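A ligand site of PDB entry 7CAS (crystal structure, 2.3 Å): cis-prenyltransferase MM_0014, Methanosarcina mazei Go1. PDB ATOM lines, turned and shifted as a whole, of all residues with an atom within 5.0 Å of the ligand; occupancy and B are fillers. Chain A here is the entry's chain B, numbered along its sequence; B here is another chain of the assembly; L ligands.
Residues that only touch the ligand: Gly 66, Asn 25, Phe 65, Asp 23, Ser 89, Pro 22, Cys 86, Tyr 40, Gly 43, Phe 133, Phe 82, Ala 85 and Phe 64. Within 4 Å of the ligand: Pro 22, Asp 23, Asn 25, Tyr 40, Gly 43, Phe 64, Phe 65, Gly 66, Asn 71, Phe 82, Ala 85, Cys 86, Ser 89, Phe 133, Arg 173, Arg 177, Ser 181 and Gly 224 of chain B.
OG of Ser 181 is in hydrogen-bond range of OXT of Gly 224 of chain B (2.5 Å). The backbone carbonyl oxygen (O) of Arg 177 lies close to the guanidinium group (NE) of Arg 173, at 3.5 Å. O of Gly 66 lies close to SG of Cys 86 (3.6 Å). OD1 of Asn 71 lies within hydrogen-bond range of NH2 of Arg 74. The backbone carbonyl oxygen (O) of Pro 22 lies within hydrogen-bond range of the side-chain amide nitrogen (ND2) of Asn 25, at 3.0 Å. The backbone NH of Trp 200 is in hydrogen-bond range of the backbone carbonyl oxygen of Asp 23, at 3.0 Å. The backbone carbonyl oxygen (O) of Ala 85 lies within hydrogen-bond range of the side-chain hydroxyl (OG) of Ser 89 (2.6 Å). The backbone carbonyl oxygen of Gly 43 is in hydrogen-bond range of the indole nitrogen of Trp 200 (2.9 Å).
The chain-end carboxylate (O) of Gly 224 of chain B lies close to an oxygen (O1) of the ligand. O1 of the ligand is in salt-bridge range of NH2 of Arg 173, 2.8 Å away. The side-chain hydroxyl (OG) of Ser 181 is in hydrogen-bond range of an oxygen (O1) of the ligand, 2.9 Å away. An oxygen (O2) of the ligand sits close to the side-chain amide oxygen (OD1) of Asn 71 (3.2 Å). The guanidinium group of Arg 177 lies within salt-bridge range of an oxygen (O1) of the ligand (3.6 Å).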
ATOM      1  N   ILE A  21     -27.910 -11.076 -27.731  1.00  0.00           N
ATOM      2  CA  ILE A  21     -27.353 -10.920 -26.360  1.00  0.00           C
ATOM      3  C   ILE A  21     -26.157  -9.984 -26.438  1.00  0.00           C
ATOM      4  O   ILE A  21     -25.084 -10.379 -26.897  1.00  0.00           O
ATOM      5  CB  ILE A  21     -26.997 -12.296 -25.751  1.00  0.00           C
ATOM      6  CG1 ILE A  21     -28.185 -13.264 -25.816  1.00  0.00           C
ATOM      7  CG2 ILE A  21     -26.477 -12.127 -24.319  1.00  0.00           C
ATOM      8  CD1 ILE A  21     -28.082 -14.443 -24.867  1.00  0.00           C
ATOM      9  N   PRO A  22     -26.333  -8.700 -26.062  1.00  0.00           N
ATOM     10  CA  PRO A  22     -25.289  -7.692 -26.234  1.00  0.00           C
ATOM     11  C   PRO A  22     -24.343  -7.647 -25.025  1.00  0.00           C
ATOM     12  O   PRO A  22     -24.351  -6.655 -24.317  1.00  0.00           O
ATOM     13  CB  PRO A  22     -26.110  -6.407 -26.362  1.00  0.00           C
ATOM     14  CG  PRO A  22     -27.305  -6.648 -25.426  1.00  0.00           C
ATOM     15  CD  PRO A  22     -27.559  -8.147 -25.482  1.00  0.00           C
ATOM     16  N   ASP A  23     -23.606  -8.728 -24.800  1.00  0.00           N
ATOM     17  CA  ASP A  23     -22.778  -8.961 -23.585  1.00  0.00           C
ATOM     18  C   ASP A  23     -21.338  -8.518 -23.876  1.00  0.00           C
ATOM     19  O   ASP A  23     -20.968  -8.433 -25.054  1.00  0.00           O
ATOM     20  CB  ASP A  23     -22.843 -10.424 -23.151  1.00  0.00           C
ATOM     21  CG  ASP A  23     -22.413 -10.642 -21.706  1.00  0.00           C
ATOM     22  OD1 ASP A  23     -22.755  -9.788 -20.853  1.00  0.00           O
ATOM     23  OD2 ASP A  23     -21.737 -11.666 -21.448  1.00  0.00           O
ATOM     24  N   ASN A  25     -19.896  -5.708 -22.106  1.00  0.00           N
ATOM     25  CA  ASN A  25     -19.852  -4.247 -21.874  1.00  0.00           C
ATOM     26  C   ASN A  25     -18.793  -3.927 -20.805  1.00  0.00           C
ATOM     27  O   ASN A  25     -17.987  -3.002 -21.022  1.00  0.00           O
ATOM     28  CB  ASN A  25     -21.218  -3.699 -21.489  1.00  0.00           C
ATOM     29  CG  ASN A  25     -22.274  -3.972 -22.527  1.00  0.00           C
ATOM     30  OD1 ASN A  25     -22.245  -3.396 -23.605  1.00  0.00           O
ATOM     31  ND2 ASN A  25     -23.187  -4.890 -22.234  1.00  0.00           N
ATOM     32  N   TYR A  40     -21.612   0.350 -20.807  1.00  0.00           N
ATOM     33  CA  TYR A  40     -23.020   0.066 -21.212  1.00  0.00           C
ATOM     34  C   TYR A  40     -23.490   1.137 -22.209  1.00  0.00           C
ATOM     35  O   TYR A  40     -24.037   0.763 -23.268  1.00  0.00           O
ATOM     36  CB  TYR A  40     -23.925  -0.005 -19.983  1.00  0.00           C
ATOM     37  CG  TYR A  40     -23.703  -1.232 -19.127  1.00  0.00           C
ATOM     38  CD1 TYR A  40     -23.943  -2.503 -19.624  1.00  0.00           C
ATOM     39  CD2 TYR A  40     -23.231  -1.118 -17.825  1.00  0.00           C
ATOM     40  CE1 TYR A  40     -23.722  -3.634 -18.848  1.00  0.00           C
ATOM     41  CE2 TYR A  40     -23.008  -2.237 -17.041  1.00  0.00           C
ATOM     42  CZ  TYR A  40     -23.258  -3.503 -17.558  1.00  0.00           C
ATOM     43  OH  TYR A  40     -23.044  -4.605 -16.786  1.00  0.00           O
ATOM     44  N   GLY A  43     -23.021   0.790 -25.712  1.00  0.00           N
ATOM     45  CA  GLY A  43     -23.813  -0.325 -26.255  1.00  0.00           C
ATOM     46  C   GLY A  43     -24.982   0.162 -27.094  1.00  0.00           C
ATOM     47  O   GLY A  43     -25.553  -0.650 -27.829  1.00  0.00           O
ATOM     48  N   ILE A  44     -25.320   1.461 -26.993  1.00  0.00           N
ATOM     49  CA  ILE A  44     -26.588   2.036 -27.521  1.00  0.00           C
ATOM     50  C   ILE A  44     -26.535   2.071 -29.053  1.00  0.00           C
ATOM     51  O   ILE A  44     -27.461   1.548 -29.691  1.00  0.00           O
ATOM     52  CB  ILE A  44     -26.856   3.428 -26.917  1.00  0.00           C
ATOM     53  CG1 ILE A  44     -26.951   3.381 -25.389  1.00  0.00           C
ATOM     54  CG2 ILE A  44     -28.097   4.069 -27.535  1.00  0.00           C
ATOM     55  CD1 ILE A  44     -26.879   4.730 -24.713  1.00  0.00           C
ATOM     56  N   GLY A  47     -26.674  -1.221 -31.035  1.00  0.00           N
ATOM     57  CA  GLY A  47     -28.107  -1.573 -31.108  1.00  0.00           C
ATOM     58  C   GLY A  47     -28.767  -0.952 -32.331  1.00  0.00           C
ATOM     59  O   GLY A  47     -29.505  -1.672 -33.035  1.00  0.00           O
ATOM     60  N   PHE A  64     -33.951  -8.150 -28.510  1.00  0.00           N
ATOM     61  CA  PHE A  64     -32.777  -7.708 -27.734  1.00  0.00           C
ATOM     62  C   PHE A  64     -32.928  -8.185 -26.285  1.00  0.00           C
ATOM     63  O   PHE A  64     -34.002  -7.994 -25.699  1.00  0.00           O
ATOM     64  CB  PHE A  64     -32.615  -6.190 -27.813  1.00  0.00           C
ATOM     65  CG  PHE A  64     -32.126  -5.679 -29.139  1.00  0.00           C
ATOM     66  CD1 PHE A  64     -30.778  -5.747 -29.463  1.00  0.00           C
ATOM     67  CD2 PHE A  64     -33.013  -5.141 -30.068  1.00  0.00           C
ATOM     68  CE1 PHE A  64     -30.330  -5.275 -30.690  1.00  0.00           C
ATOM     69  CE2 PHE A  64     -32.549  -4.674 -31.288  1.00  0.00           C
ATOM     70  CZ  PHE A  64     -31.214  -4.753 -31.594  1.00  0.00           C
ATOM     71  N   PHE A  65     -31.909  -8.865 -25.767  1.00  0.00           N
ATOM     72  CA  PHE A  65     -31.643  -9.061 -24.328  1.00  0.00           C
ATOM     73  C   PHE A  65     -31.242  -7.717 -23.712  1.00  0.00           C
ATOM     74  O   PHE A  65     -30.133  -7.247 -23.977  1.00  0.00           O
ATOM     75  CB  PHE A  65     -30.561 -10.130 -24.140  1.00  0.00           C
ATOM     76  CG  PHE A  65     -30.323 -10.575 -22.708  1.00  0.00           C
ATOM     77  CD1 PHE A  65     -29.957  -9.655 -21.735  1.00  0.00           C
ATOM     78  CD2 PHE A  65     -30.362 -11.919 -22.366  1.00  0.00           C
ATOM     79  CE1 PHE A  65     -29.696 -10.075 -20.433  1.00  0.00           C
ATOM     80  CE2 PHE A  65     -30.108 -12.327 -21.068  1.00  0.00           C
ATOM     81  CZ  PHE A  65     -29.765 -11.402 -20.113  1.00  0.00           C
ATOM     82  N   GLY A  66     -32.179  -7.072 -23.002  1.00  0.00           N
ATOM     83  CA  GLY A  66     -31.947  -5.801 -22.299  1.00  0.00           C
ATOM     84  C   GLY A  66     -31.245  -6.021 -20.979  1.00  0.00           C
ATOM     85  O   GLY A  66     -30.019  -5.855 -20.927  1.00  0.00           O
ATOM     86  N   PHE A  67     -31.996  -6.412 -19.946  1.00  0.00           N
ATOM     87  CA  PHE A  67     -31.467  -6.963 -18.675  1.00  0.00           C
ATOM     88  C   PHE A  67     -32.519  -7.875 -18.049  1.00  0.00           C
ATOM     89  O   PHE A  67     -33.706  -7.788 -18.430  1.00  0.00           O
ATOM     90  CB  PHE A  67     -31.034  -5.842 -17.729  1.00  0.00           C
ATOM     91  CG  PHE A  67     -32.162  -5.022 -17.148  1.00  0.00           C
ATOM     92  CD1 PHE A  67     -32.786  -5.416 -15.972  1.00  0.00           C
ATOM     93  CD2 PHE A  67     -32.550  -3.825 -17.730  1.00  0.00           C
ATOM     94  CE1 PHE A  67     -33.802  -4.636 -15.417  1.00  0.00           C
ATOM     95  CE2 PHE A  67     -33.574  -3.063 -17.186  1.00  0.00           C
ATOM     96  CZ  PHE A  67     -34.193  -3.475 -16.022  1.00  0.00           C
ATOM     97  N   ASN A  71     -29.708  -9.845 -13.337  1.00  0.00           N
ATOM     98  CA  ASN A  71     -28.745  -8.742 -13.618  1.00  0.00           C
ATOM     99  C   ASN A  71     -28.904  -7.639 -12.554  1.00  0.00           C
ATOM    100  O   ASN A  71     -27.919  -6.922 -12.312  1.00  0.00           O
ATOM    101  CB  ASN A  71     -28.953  -8.163 -15.023  1.00  0.00           C
ATOM    102  CG  ASN A  71     -28.500  -9.103 -16.127  1.00  0.00           C
ATOM    103  OD1 ASN A  71     -27.604  -9.912 -15.928  1.00  0.00           O
ATOM    104  ND2 ASN A  71     -29.089  -8.972 -17.301  1.00  0.00           N
ATOM    105  N   ARG A  74     -26.566  -7.317  -9.478  1.00  0.00           N
ATOM    106  CA  ARG A  74     -25.233  -6.683  -9.690  1.00  0.00           C
ATOM    107  C   ARG A  74     -25.225  -5.299  -9.022  1.00  0.00           C
ATOM    108  O   ARG A  74     -26.282  -4.734  -8.753  1.00  0.00           O
ATOM    109  CB  ARG A  74     -24.922  -6.599 -11.190  1.00  0.00           C
ATOM    110  CG  ARG A  74     -25.136  -7.900 -11.940  1.00  0.00           C
ATOM    111  CD  ARG A  74     -23.932  -8.337 -12.742  1.00  0.00           C
ATOM    112  NE  ARG A  74     -23.996  -7.895 -14.132  1.00  0.00           N
ATOM    113  CZ  ARG A  74     -24.136  -8.699 -15.183  1.00  0.00           C
ATOM    114  NH1 ARG A  74     -24.184  -8.184 -16.405  1.00  0.00           N
ATOM    115  NH2 ARG A  74     -24.228 -10.013 -15.021  1.00  0.00           N
ATOM    116  N   PHE A  82     -26.873   0.171 -17.150  1.00  0.00           N
ATOM    117  CA  PHE A  82     -27.437  -0.734 -18.191  1.00  0.00           C
ATOM    118  C   PHE A  82     -28.944  -0.482 -18.332  1.00  0.00           C
ATOM    119  O   PHE A  82     -29.462  -0.603 -19.453  1.00  0.00           O
ATOM    120  CB  PHE A  82     -27.071  -2.204 -17.926  1.00  0.00           C
ATOM    121  CG  PHE A  82     -27.705  -2.857 -16.718  1.00  0.00           C
ATOM    122  CD1 PHE A  82     -29.094  -2.973 -16.611  1.00  0.00           C
ATOM    123  CD2 PHE A  82     -26.924  -3.506 -15.780  1.00  0.00           C
ATOM    124  CE1 PHE A  82     -29.662  -3.623 -15.528  1.00  0.00           C
ATOM    125  CE2 PHE A  82     -27.500  -4.173 -14.709  1.00  0.00           C
ATOM    126  CZ  PHE A  82     -28.866  -4.226 -14.585  1.00  0.00           C
ATOM    127  N   ALA A  85     -28.971   2.800 -20.313  1.00  0.00           N
ATOM    128  CA  ALA A  85     -28.523   2.374 -21.663  1.00  0.00           C
ATOM    129  C   ALA A  85     -29.683   1.685 -22.390  1.00  0.00           C
ATOM    130  O   ALA A  85     -29.897   1.981 -23.574  1.00  0.00           O
ATOM    131  CB  ALA A  85     -27.321   1.467 -21.548  1.00  0.00           C
ATOM    132  N   CYS A  86     -30.415   0.812 -21.696  1.00  0.00           N
ATOM    133  CA  CYS A  86     -31.605   0.082 -22.218  1.00  0.00           C
ATOM    134  C   CYS A  86     -32.715   1.083 -22.558  1.00  0.00           C
ATOM    135  O   CYS A  86     -33.216   1.042 -23.711  1.00  0.00           O
ATOM    136  CB  CYS A  86     -32.114  -0.944 -21.202  1.00  0.00           C
ATOM    137  SG  CYS A  86     -31.194  -2.515 -21.241  1.00  0.00           S
ATOM    138  N   SER A  89     -31.870   3.019 -25.584  1.00  0.00           N
ATOM    139  CA  SER A  89     -31.862   2.075 -26.744  1.00  0.00           C
ATOM    140  C   SER A  89     -33.291   1.908 -27.285  1.00  0.00           C
ATOM    141  O   SER A  89     -33.473   2.018 -28.513  1.00  0.00           O
ATOM    142  CB  SER A  89     -31.272   0.748 -26.355  1.00  0.00           C
ATOM    143  OG  SER A  89     -29.949   0.900 -25.886  1.00  0.00           O
ATOM    144  N   PHE A 133     -37.718  -6.037 -26.649  1.00  0.00           N
ATOM    145  CA  PHE A 133     -36.721  -5.827 -25.575  1.00  0.00           C
ATOM    146  C   PHE A 133     -37.131  -6.610 -24.333  1.00  0.00           C
ATOM    147  O   PHE A 133     -38.292  -6.493 -23.909  1.00  0.00           O
ATOM    148  CB  PHE A 133     -36.591  -4.335 -25.257  1.00  0.00           C
ATOM    149  CG  PHE A 133     -36.086  -3.491 -26.396  1.00  0.00           C
ATOM    150  CD1 PHE A 133     -36.966  -2.946 -27.321  1.00  0.00           C
ATOM    151  CD2 PHE A 133     -34.730  -3.213 -26.536  1.00  0.00           C
ATOM    152  CE1 PHE A 133     -36.500  -2.158 -28.360  1.00  0.00           C
ATOM    153  CE2 PHE A 133     -34.280  -2.419 -27.582  1.00  0.00           C
ATOM    154  CZ  PHE A 133     -35.164  -1.897 -28.486  1.00  0.00           C
ATOM    155  N   ARG A 173     -24.701 -13.853 -29.671  1.00  0.00           N
ATOM    156  CA  ARG A 173     -24.188 -13.346 -28.374  1.00  0.00           C
ATOM    157  C   ARG A 173     -22.775 -12.786 -28.571  1.00  0.00           C
ATOM    158  O   ARG A 173     -21.940 -13.487 -29.164  1.00  0.00           O
ATOM    159  CB  ARG A 173     -24.183 -14.472 -27.331  1.00  0.00           C
ATOM    160  CG  ARG A 173     -23.519 -14.097 -26.016  1.00  0.00           C
ATOM    161  CD  ARG A 173     -24.050 -14.877 -24.844  1.00  0.00           C
ATOM    162  NE  ARG A 173     -23.547 -14.360 -23.575  1.00  0.00           N
ATOM    163  CZ  ARG A 173     -24.123 -14.562 -22.395  1.00  0.00           C
ATOM    164  NH1 ARG A 173     -25.234 -15.284 -22.314  1.00  0.00           N
ATOM    165  NH2 ARG A 173     -23.594 -14.031 -21.301  1.00  0.00           N
ATOM    166  N   ARG A 177     -18.846 -15.677 -24.543  1.00  0.00           N
ATOM    167  CA  ARG A 177     -19.521 -16.703 -23.704  1.00  0.00           C
ATOM    168  C   ARG A 177     -20.652 -17.358 -24.496  1.00  0.00           C
ATOM    169  O   ARG A 177     -21.427 -16.627 -25.136  1.00  0.00           O
ATOM    170  CB  ARG A 177     -20.069 -16.082 -22.419  1.00  0.00           C
ATOM    171  CG  ARG A 177     -19.045 -15.278 -21.625  1.00  0.00           C
ATOM    172  CD  ARG A 177     -19.638 -14.705 -20.367  1.00  0.00           C
ATOM    173  NE  ARG A 177     -20.107 -15.739 -19.458  1.00  0.00           N
ATOM    174  CZ  ARG A 177     -20.910 -15.530 -18.413  1.00  0.00           C
ATOM    175  NH1 ARG A 177     -21.352 -14.309 -18.149  1.00  0.00           N
ATOM    176  NH2 ARG A 177     -21.273 -16.549 -17.650  1.00  0.00           N
ATOM    177  N   SER A 181     -28.035 -17.381 -20.730  1.00  0.00           N
ATOM    178  CA  SER A 181     -28.238 -16.598 -19.478  1.00  0.00           C
ATOM    179  C   SER A 181     -29.742 -16.418 -19.219  1.00  0.00           C
ATOM    180  O   SER A 181     -30.152 -15.292 -18.853  1.00  0.00           O
ATOM    181  CB  SER A 181     -27.526 -15.266 -19.544  1.00  0.00           C
ATOM    182  OG  SER A 181     -26.118 -15.437 -19.604  1.00  0.00           O
ATOM    183  N   TRP A 200     -19.637  -6.445 -26.942  1.00  0.00           N
ATOM    184  CA  TRP A 200     -20.800  -5.827 -27.633  1.00  0.00           C
ATOM    185  C   TRP A 200     -20.431  -4.439 -28.160  1.00  0.00           C
ATOM    186  O   TRP A 200     -20.671  -4.126 -29.318  1.00  0.00           O
ATOM    187  CB  TRP A 200     -22.019  -5.797 -26.705  1.00  0.00           C
ATOM    188  CG  TRP A 200     -23.159  -4.968 -27.219  1.00  0.00           C
ATOM    189  CD1 TRP A 200     -23.664  -3.833 -26.655  1.00  0.00           C
ATOM    190  CD2 TRP A 200     -23.932  -5.208 -28.407  1.00  0.00           C
ATOM    191  NE1 TRP A 200     -24.712  -3.360 -27.407  1.00  0.00           N
ATOM    192  CE2 TRP A 200     -24.896  -4.177 -28.486  1.00  0.00           C
ATOM    193  CE3 TRP A 200     -23.915  -6.189 -29.399  1.00  0.00           C
ATOM    194  CZ2 TRP A 200     -25.834  -4.109 -29.522  1.00  0.00           C
ATOM    195  CZ3 TRP A 200     -24.837  -6.114 -30.420  1.00  0.00           C
ATOM    196  CH2 TRP A 200     -25.779  -5.089 -30.481  1.00  0.00           C
ATOM    197  N   GLY B 224     -24.158 -14.773 -14.080  1.00  0.00           N
ATOM    198  CA  GLY B 224     -24.998 -15.625 -14.961  1.00  0.00           C
ATOM    199  C   GLY B 224     -24.933 -15.178 -16.409  1.00  0.00           C
ATOM    200  O   GLY B 224     -24.555 -14.044 -16.709  1.00  0.00           O
ATOM    201  OXT GLY B 224     -25.250 -15.940 -17.317  1.00  0.00           O
HETATM  202  C1  LIG L   1     -25.589 -12.248 -18.966  1.00  0.00           C
HETATM  203  O1  LIG L   1     -24.650 -13.073 -18.926  1.00  0.00           O
HETATM  204  O2  LIG L   1     -26.373 -12.059 -18.022  1.00  0.00           O
HETATM  205  C2  LIG L   1     -25.778 -11.447 -20.234  1.00  0.00           C
HETATM  206  C3  LIG L   1     -26.005  -9.994 -20.016  1.00  0.00           C
HETATM  207  C4  LIG L   1     -26.511  -9.286 -21.256  1.00  0.00           C
HETATM  208  C5  LIG L   1     -27.188  -7.974 -20.992  1.00  0.00           C
HETATM  209  C6  LIG L   1     -26.244  -6.878 -20.575  1.00  0.00           C
HETATM  210  C7  LIG L   1     -26.304  -5.662 -21.442  1.00  0.00           C
HETATM  211  C8  LIG L   1     -27.204  -4.571 -20.918  1.00  0.00           C
HETATM  212  C9  LIG L   1     -27.836  -3.727 -21.993  1.00  0.00           C
HETATM  213  C10 LIG L   1     -27.252  -2.334 -22.126  1.00  0.00           C
HETATM  214  C11 LIG L   1     -26.411  -2.131 -23.356  1.00  0.00           C
HETATM  215  C12 LIG L   1     -27.149  -1.504 -24.506  1.00  0.00           C
HETATM  216  C13 LIG L   1     -28.394  -2.255 -24.928  1.00  0.00           C
HETATM  217  C14 LIG L   1     -28.685  -2.193 -26.407  1.00  0.00           C
HETATM  218  C15 LIG L   1     -29.831  -3.071 -26.851  1.00  0.00           C
HETATM  219  C16 LIG L   1     -30.957  -3.160 -25.856  1.00  0.00           C
